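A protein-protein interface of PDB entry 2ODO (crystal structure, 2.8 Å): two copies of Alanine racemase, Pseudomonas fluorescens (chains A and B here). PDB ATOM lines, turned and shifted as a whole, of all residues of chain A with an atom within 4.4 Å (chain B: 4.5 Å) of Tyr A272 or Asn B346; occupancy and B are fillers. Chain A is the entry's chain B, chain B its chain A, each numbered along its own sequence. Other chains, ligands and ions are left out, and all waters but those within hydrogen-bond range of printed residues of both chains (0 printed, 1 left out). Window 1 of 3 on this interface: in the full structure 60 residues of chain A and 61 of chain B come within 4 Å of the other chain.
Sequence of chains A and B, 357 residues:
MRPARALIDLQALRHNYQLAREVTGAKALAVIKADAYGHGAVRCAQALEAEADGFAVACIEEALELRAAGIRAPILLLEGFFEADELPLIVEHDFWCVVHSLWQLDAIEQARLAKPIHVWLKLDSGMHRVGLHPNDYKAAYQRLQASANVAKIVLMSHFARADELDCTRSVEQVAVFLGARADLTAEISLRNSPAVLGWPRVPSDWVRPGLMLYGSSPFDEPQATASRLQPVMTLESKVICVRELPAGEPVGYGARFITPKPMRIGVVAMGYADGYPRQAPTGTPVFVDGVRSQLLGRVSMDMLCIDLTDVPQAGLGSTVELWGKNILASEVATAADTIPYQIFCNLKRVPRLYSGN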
ATOM      1  N   GLY A 271     -14.546  10.424  -2.182  1.00  0.00           N
ATOM      2  CA  GLY A 271     -14.811   8.989  -2.305  1.00  0.00           C
ATOM      3  C   GLY A 271     -15.894   8.661  -3.312  1.00  0.00           C
ATOM      4  O   GLY A 271     -16.391   9.553  -4.003  1.00  0.00           O
ATOM      5  N   TYR A 272     -16.266   7.383  -3.394  1.00  0.00           N
ATOM      6  CA  TYR A 272     -17.288   6.957  -4.356  1.00  0.00           C
ATOM      7  C   TYR A 272     -18.711   7.362  -3.985  1.00  0.00           C
ATOM      8  O   TYR A 272     -19.594   7.409  -4.845  1.00  0.00           O
ATOM      9  CB  TYR A 272     -17.188   5.462  -4.719  1.00  0.00           C
ATOM     10  CG  TYR A 272     -17.196   4.467  -3.573  1.00  0.00           C
ATOM     11  CD1 TYR A 272     -16.030   3.804  -3.202  1.00  0.00           C
ATOM     12  CD2 TYR A 272     -18.374   4.157  -2.891  1.00  0.00           C
ATOM     13  CE1 TYR A 272     -16.026   2.878  -2.166  1.00  0.00           C
ATOM     14  CE2 TYR A 272     -18.380   3.231  -1.847  1.00  0.00           C
ATOM     15  CZ  TYR A 272     -17.200   2.595  -1.493  1.00  0.00           C
ATOM     16  OH  TYR A 272     -17.187   1.677  -0.469  1.00  0.00           O
ATOM     17  N   ALA A 273     -18.920   7.665  -2.706  1.00  0.00           N
ATOM     18  CA  ALA A 273     -20.199   8.180  -2.221  1.00  0.00           C
ATOM     19  C   ALA A 273     -20.438   9.607  -2.706  1.00  0.00           C
ATOM     20  O   ALA A 273     -21.583  10.024  -2.888  1.00  0.00           O
ATOM     21  CB  ALA A 273     -20.252   8.125  -0.709  1.00  0.00           C
ATOM     22  N   ASP A 274     -19.348  10.343  -2.907  1.00  0.00           N
ATOM     23  CA  ASP A 274     -19.400  11.720  -3.393  1.00  0.00           C
ATOM     24  C   ASP A 274     -19.726  11.779  -4.881  1.00  0.00           C
ATOM     25  O   ASP A 274     -20.243  12.786  -5.368  1.00  0.00           O
ATOM     26  CB  ASP A 274     -18.070  12.424  -3.132  1.00  0.00           C
ATOM     27  CG  ASP A 274     -17.694  12.439  -1.666  1.00  0.00           C
ATOM     28  OD1 ASP A 274     -18.386  13.113  -0.875  1.00  0.00           O
ATOM     29  OD2 ASP A 274     -16.698  11.782  -1.306  1.00  0.00           O
ATOM     30  N   GLY A 275     -19.412  10.702  -5.597  1.00  0.00           N
ATOM     31  CA  GLY A 275     -19.691  10.614  -7.025  1.00  0.00           C
ATOM     32  C   GLY A 275     -18.524  10.143  -7.867  1.00  0.00           C
ATOM     33  O   GLY A 275     -18.688   9.888  -9.060  1.00  0.00           O
ATOM     34  N   TYR A 276     -17.346  10.033  -7.255  1.00  0.00           N
ATOM     35  CA  TYR A 276     -16.153   9.566  -7.960  1.00  0.00           C
ATOM     36  C   TYR A 276     -16.236   8.060  -8.210  1.00  0.00           C
ATOM     37  O   TYR A 276     -16.524   7.300  -7.289  1.00  0.00           O
ATOM     38  CB  TYR A 276     -14.879   9.909  -7.179  1.00  0.00           C
ATOM     39  CG  TYR A 276     -13.625   9.841  -8.022  1.00  0.00           C
ATOM     40  CD1 TYR A 276     -13.218  10.935  -8.785  1.00  0.00           C
ATOM     41  CD2 TYR A 276     -12.854   8.682  -8.071  1.00  0.00           C
ATOM     42  CE1 TYR A 276     -12.074  10.881  -9.569  1.00  0.00           C
ATOM     43  CE2 TYR A 276     -11.704   8.617  -8.855  1.00  0.00           C
ATOM     44  CZ  TYR A 276     -11.322   9.721  -9.601  1.00  0.00           C
ATOM     45  OH  TYR A 276     -10.187   9.668 -10.378  1.00  0.00           O
ATOM     46  N   ARG A 278     -15.631   4.259  -8.407  1.00  0.00           N
ATOM     47  CA  ARG A 278     -14.790   3.247  -7.769  1.00  0.00           C
ATOM     48  C   ARG A 278     -14.106   2.388  -8.832  1.00  0.00           C
ATOM     49  O   ARG A 278     -13.044   1.808  -8.587  1.00  0.00           O
ATOM     50  CB  ARG A 278     -15.615   2.367  -6.825  1.00  0.00           C
ATOM     51  CG  ARG A 278     -14.794   1.366  -6.019  1.00  0.00           C
ATOM     52  CD  ARG A 278     -15.671   0.408  -5.233  1.00  0.00           C
ATOM     53  NE  ARG A 278     -14.872  -0.627  -4.578  1.00  0.00           N
ATOM     54  CZ  ARG A 278     -14.713  -1.867  -5.037  1.00  0.00           C
ATOM     55  NH1 ARG A 278     -15.309  -2.253  -6.160  1.00  0.00           N
ATOM     56  NH2 ARG A 278     -13.963  -2.728  -4.365  1.00  0.00           N
ATOM     57  N   VAL A 299     -10.548   3.043  -4.305  1.00  0.00           N
ATOM     58  CA  VAL A 299     -11.219   4.235  -3.803  1.00  0.00           C
ATOM     59  C   VAL A 299     -12.131   3.814  -2.653  1.00  0.00           C
ATOM     60  O   VAL A 299     -12.925   2.879  -2.795  1.00  0.00           O
ATOM     61  CB  VAL A 299     -12.032   4.946  -4.924  1.00  0.00           C
ATOM     62  CG1 VAL A 299     -12.773   6.165  -4.383  1.00  0.00           C
ATOM     63  CG2 VAL A 299     -11.120   5.353  -6.080  1.00  0.00           C
ATOM     64  N   SER A 300     -11.992   4.488  -1.512  1.00  0.00           N
ATOM     65  CA  SER A 300     -12.864   4.258  -0.362  1.00  0.00           C
ATOM     66  C   SER A 300     -14.152   5.069  -0.506  1.00  0.00           C
ATOM     67  O   SER A 300     -14.300   5.854  -1.446  1.00  0.00           O
ATOM     68  CB  SER A 300     -12.148   4.615   0.943  1.00  0.00           C
ATOM     69  OG  SER A 300     -10.872   4.005   1.017  1.00  0.00           O
ATOM     70  N   MET A 301     -15.080   4.874   0.428  1.00  0.00           N
ATOM     71  CA  MET A 301     -16.371   5.559   0.412  1.00  0.00           C
ATOM     72  C   MET A 301     -16.240   7.085   0.483  1.00  0.00           C
ATOM     73  O   MET A 301     -16.995   7.802  -0.176  1.00  0.00           O
ATOM     74  CB  MET A 301     -17.250   5.043   1.555  1.00  0.00           C
ATOM     75  CG  MET A 301     -18.718   5.424   1.451  1.00  0.00           C
ATOM     76  SD  MET A 301     -19.745   4.554   2.650  1.00  0.00           S
ATOM     77  CE  MET A 301     -19.845   2.933   1.900  1.00  0.00           C
ATOM     78  N   ASN A 346     -23.836  10.789 -10.554  1.00  0.00           N
ATOM     79  CA  ASN A 346     -23.478  10.183  -9.273  1.00  0.00           C
ATOM     80  C   ASN A 346     -23.077  11.189  -8.191  1.00  0.00           C
ATOM     81  O   ASN A 346     -22.922  10.819  -7.024  1.00  0.00           O
ATOM     82  CB  ASN A 346     -22.376   9.132  -9.463  1.00  0.00           C
ATOM     83  CG  ASN A 346     -22.874   7.873 -10.160  1.00  0.00           C
ATOM     84  OD1 ASN A 346     -24.072   7.590 -10.189  1.00  0.00           O
ATOM     85  ND2 ASN A 346     -21.946   7.106 -10.719  1.00  0.00           N
ATOM     86  N   ASP B 274     -30.546   7.115 -10.813  1.00  0.00           N
ATOM     87  CA  ASP B 274     -31.264   6.733  -9.602  1.00  0.00           C
ATOM     88  C   ASP B 274     -30.368   5.950  -8.647  1.00  0.00           C
ATOM     89  O   ASP B 274     -30.640   5.882  -7.447  1.00  0.00           O
ATOM     90  CB  ASP B 274     -32.503   5.904  -9.951  1.00  0.00           C
ATOM     91  CG  ASP B 274     -33.483   6.656 -10.832  1.00  0.00           C
ATOM     92  OD1 ASP B 274     -34.017   7.693 -10.388  1.00  0.00           O
ATOM     93  OD2 ASP B 274     -33.729   6.201 -11.968  1.00  0.00           O
ATOM     94  N   GLY B 275     -29.306   5.354  -9.188  1.00  0.00           N
ATOM     95  CA  GLY B 275     -28.353   4.589  -8.393  1.00  0.00           C
ATOM     96  C   GLY B 275     -28.105   3.177  -8.887  1.00  0.00           C
ATOM     97  O   GLY B 275     -27.251   2.471  -8.348  1.00  0.00           O
ATOM     98  N   ILE B 339     -18.794  -3.653  -5.385  1.00  0.00           N
ATOM     99  CA  ILE B 339     -19.265  -4.052  -4.058  1.00  0.00           C
ATOM    100  C   ILE B 339     -20.581  -3.344  -3.706  1.00  0.00           C
ATOM    101  O   ILE B 339     -20.833  -2.243  -4.198  1.00  0.00           O
ATOM    102  CB  ILE B 339     -18.188  -3.799  -2.969  1.00  0.00           C
ATOM    103  CG1 ILE B 339     -17.672  -2.353  -3.033  1.00  0.00           C
ATOM    104  CG2 ILE B 339     -17.049  -4.815  -3.110  1.00  0.00           C
ATOM    105  CD1 ILE B 339     -16.673  -1.978  -1.947  1.00  0.00           C
ATOM    106  N   TYR B 341     -21.501  -1.725  -1.191  1.00  0.00           N
ATOM    107  CA  TYR B 341     -21.220  -0.412  -0.605  1.00  0.00           C
ATOM    108  C   TYR B 341     -21.560   0.734  -1.560  1.00  0.00           C
ATOM    109  O   TYR B 341     -22.295   1.656  -1.201  1.00  0.00           O
ATOM    110  CB  TYR B 341     -19.741  -0.298  -0.234  1.00  0.00           C
ATOM    111  CG  TYR B 341     -19.274  -1.161   0.917  1.00  0.00           C
ATOM    112  CD1 TYR B 341     -18.820  -2.461   0.701  1.00  0.00           C
ATOM    113  CD2 TYR B 341     -19.249  -0.664   2.218  1.00  0.00           C
ATOM    114  CE1 TYR B 341     -18.369  -3.250   1.751  1.00  0.00           C
ATOM    115  CE2 TYR B 341     -18.802  -1.444   3.275  1.00  0.00           C
ATOM    116  CZ  TYR B 341     -18.366  -2.736   3.036  1.00  0.00           C
ATOM    117  OH  TYR B 341     -17.926  -3.509   4.083  1.00  0.00           O
ATOM    118  N   GLN B 342     -21.018   0.651  -2.775  1.00  0.00           N
ATOM    119  CA  GLN B 342     -21.091   1.723  -3.768  1.00  0.00           C
ATOM    120  C   GLN B 342     -22.498   1.966  -4.319  1.00  0.00           C
ATOM    121  O   GLN B 342     -22.954   3.111  -4.361  1.00  0.00           O
ATOM    122  CB  GLN B 342     -20.112   1.444  -4.914  1.00  0.00           C
ATOM    123  CG  GLN B 342     -19.973   2.580  -5.920  1.00  0.00           C
ATOM    124  CD  GLN B 342     -19.261   2.162  -7.196  1.00  0.00           C
ATOM    125  OE1 GLN B 342     -19.288   0.994  -7.588  1.00  0.00           O
ATOM    126  NE2 GLN B 342     -18.628   3.123  -7.858  1.00  0.00           N
ATOM    127  N   ILE B 343     -23.173   0.896  -4.740  1.00  0.00           N
ATOM    128  CA  ILE B 343     -24.506   1.015  -5.347  1.00  0.00           C
ATOM    129  C   ILE B 343     -25.572   1.502  -4.364  1.00  0.00           C
ATOM    130  O   ILE B 343     -26.587   2.068  -4.773  1.00  0.00           O
ATOM    131  CB  ILE B 343     -24.963  -0.289  -6.062  1.00  0.00           C
ATOM    132  CG1 ILE B 343     -24.988  -1.480  -5.095  1.00  0.00           C
ATOM    133  CG2 ILE B 343     -24.074  -0.568  -7.276  1.00  0.00           C
ATOM    134  CD1 ILE B 343     -25.810  -2.660  -5.586  1.00  0.00           C
ATOM    135  N   PHE B 344     -25.330   1.277  -3.072  1.00  0.00           N
ATOM    136  CA  PHE B 344     -26.175   1.820  -2.011  1.00  0.00           C
ATOM    137  C   PHE B 344     -26.026   3.338  -1.925  1.00  0.00           C
ATOM    138  O   PHE B 344     -27.023   4.061  -1.846  1.00  0.00           O
ATOM    139  CB  PHE B 344     -25.829   1.190  -0.657  1.00  0.00           C
ATOM    140  CG  PHE B 344     -26.424  -0.179  -0.437  1.00  0.00           C
ATOM    141  CD1 PHE B 344     -25.725  -1.137   0.290  1.00  0.00           C
ATOM    142  CD2 PHE B 344     -27.680  -0.509  -0.945  1.00  0.00           C
ATOM    143  CE1 PHE B 344     -26.259  -2.401   0.507  1.00  0.00           C
ATOM    144  CE2 PHE B 344     -28.223  -1.773  -0.734  1.00  0.00           C
ATOM    145  CZ  PHE B 344     -27.511  -2.719  -0.005  1.00  0.00           C
ATOM    146  N   CYS B 345     -24.777   3.807  -1.946  1.00  0.00           N
ATOM    147  CA  CYS B 345     -24.457   5.234  -1.867  1.00  0.00           C
ATOM    148  C   CYS B 345     -24.936   6.025  -3.082  1.00  0.00           C
ATOM    149  O   CYS B 345     -25.265   7.204  -2.963  1.00  0.00           O
ATOM    150  CB  CYS B 345     -22.952   5.440  -1.692  1.00  0.00           C
ATOM    151  SG  CYS B 345     -22.293   4.872  -0.115  1.00  0.00           S
ATOM    152  N   ASN B 346     -24.972   5.370  -4.242  1.00  0.00           N
ATOM    153  CA  ASN B 346     -25.376   6.014  -5.494  1.00  0.00           C
ATOM    154  C   ASN B 346     -26.862   6.359  -5.580  1.00  0.00           C
ATOM    155  O   ASN B 346     -27.282   7.068  -6.500  1.00  0.00           O
ATOM    156  CB  ASN B 346     -24.977   5.149  -6.697  1.00  0.00           C
ATOM    157  CG  ASN B 346     -23.479   5.144  -6.951  1.00  0.00           C
ATOM    158  OD1 ASN B 346     -22.735   5.962  -6.409  1.00  0.00           O
ATOM    159  ND2 ASN B 346     -23.032   4.218  -7.791  1.00  0.00           N
ATOM    160  N   LEU B 347     -27.649   5.867  -4.622  1.00  0.00           N
ATOM    161  CA  LEU B 347     -29.101   6.054  -4.630  1.00  0.00           C
ATOM    162  C   LEU B 347     -29.492   7.528  -4.641  1.00  0.00           C
ATOM    163  O   LEU B 347     -29.056   8.301  -3.791  1.00  0.00           O
ATOM    164  CB  LEU B 347     -29.758   5.335  -3.446  1.00  0.00           C
ATOM    165  CG  LEU B 347     -31.278   5.156  -3.543  1.00  0.00           C
ATOM    166  CD1 LEU B 347     -31.620   3.937  -4.382  1.00  0.00           C
ATOM    167  CD2 LEU B 347     -31.900   5.042  -2.166  1.00  0.00           C
ATOM    168  N   LYS B 348     -30.320   7.897  -5.614  1.00  0.00           N
ATOM    169  CA  LYS B 348     -30.722   9.285  -5.831  1.00  0.00           C
ATOM    170  C   LYS B 348     -32.136   9.390  -6.387  1.00  0.00           C
ATOM    171  O   LYS B 348     -32.682   8.411  -6.902  1.00  0.00           O
ATOM    172  CB  LYS B 348     -29.762   9.959  -6.808  1.00  0.00           C
ATOM    173  CG  LYS B 348     -28.677  10.791  -6.174  1.00  0.00           C
ATOM    174  CD  LYS B 348     -27.861  11.456  -7.259  1.00  0.00           C
ATOM    175  CE  LYS B 348     -27.613  12.916  -6.950  1.00  0.00           C
ATOM    176  NZ  LYS B 348     -27.033  13.622  -8.125  1.00  0.00           N
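OH of Tyr A272 touches CD1 of Ile B339, 3.98 Å away. Tyr B341 touches Tyr A272 (CB to OH, 3.2 Å). CA of Gln B342 touches CE2 of Tyr A272 (3.6 Å). Tyr A272 touches Asn B346. Ala A273 touches Cys B345. Ile B339 touches Arg A278. Tyr B341 touches Met A301.
3 positions are printed for both chains. Of the 9 pairs that touch across the chains among the printed residues, none has its exchanged pair printed and touching as well.
N of Arg A278 lies close to NE2 of Gln B342 (3.3 Å). The side-chain sulfur of Met A301 lies close to the side-chain sulfur of Cys B345, 3.8 Å away.
Of the 11 printed residues of chain B, 5 touch a printed residue of chain A. Among the printed residues, 9 pairs touch across the chains.
The side-chain sulfur (SG) of Cys B345 is in hydrogen-bond range of the backbone carbonyl oxygen (O) of Tyr B341 (3.4 Å). N of Tyr A272 is in hydrogen-bond range of O of Ser A300. The backbone NH (N) of Tyr A272 sits at hydrogen-bond distance from the backbone carbonyl oxygen (O) of Met A301, 3.3 Å away. The backbone NH (N) of Ala A273 is in hydrogen-bond range of the backbone carbonyl oxygen (O) of Met A301.
Of chain B, only Ile B339 (3.98 Å), Tyr B341 (3.2 Å), Gln B342 (3.6 Å) and Asn B346 (3.8 Å) come within 4 Å of Tyr A272. Printed residues of chain B within 4 Å of Ala A273: Cys B345. Printed residues of chain B within 4 Å of Arg A278: Ile B339 (3.5 Å) and Gln B342 (3.3 Å). Ser A300 touches none of the printed residues of chain B. Of the printed residues of chain B, Met A301 touches Tyr B341 and Cys B345. Gly B275 touches none of the printed residues of chain A. Printed residues of chain A within 4 Å of Ile B339: Tyr A272 (3.98 Å) and Arg A278 (3.5 Å). Printed residues of chain A within 4 Å of Tyr B341: Tyr A272 and Met A301. Of chain A, only Tyr A272 (3.8 Å) comes within 4 Å of Asn B346. The nearest printed residue of chain B that does not touch Met A301 is Gln B342 (5.3 Å).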
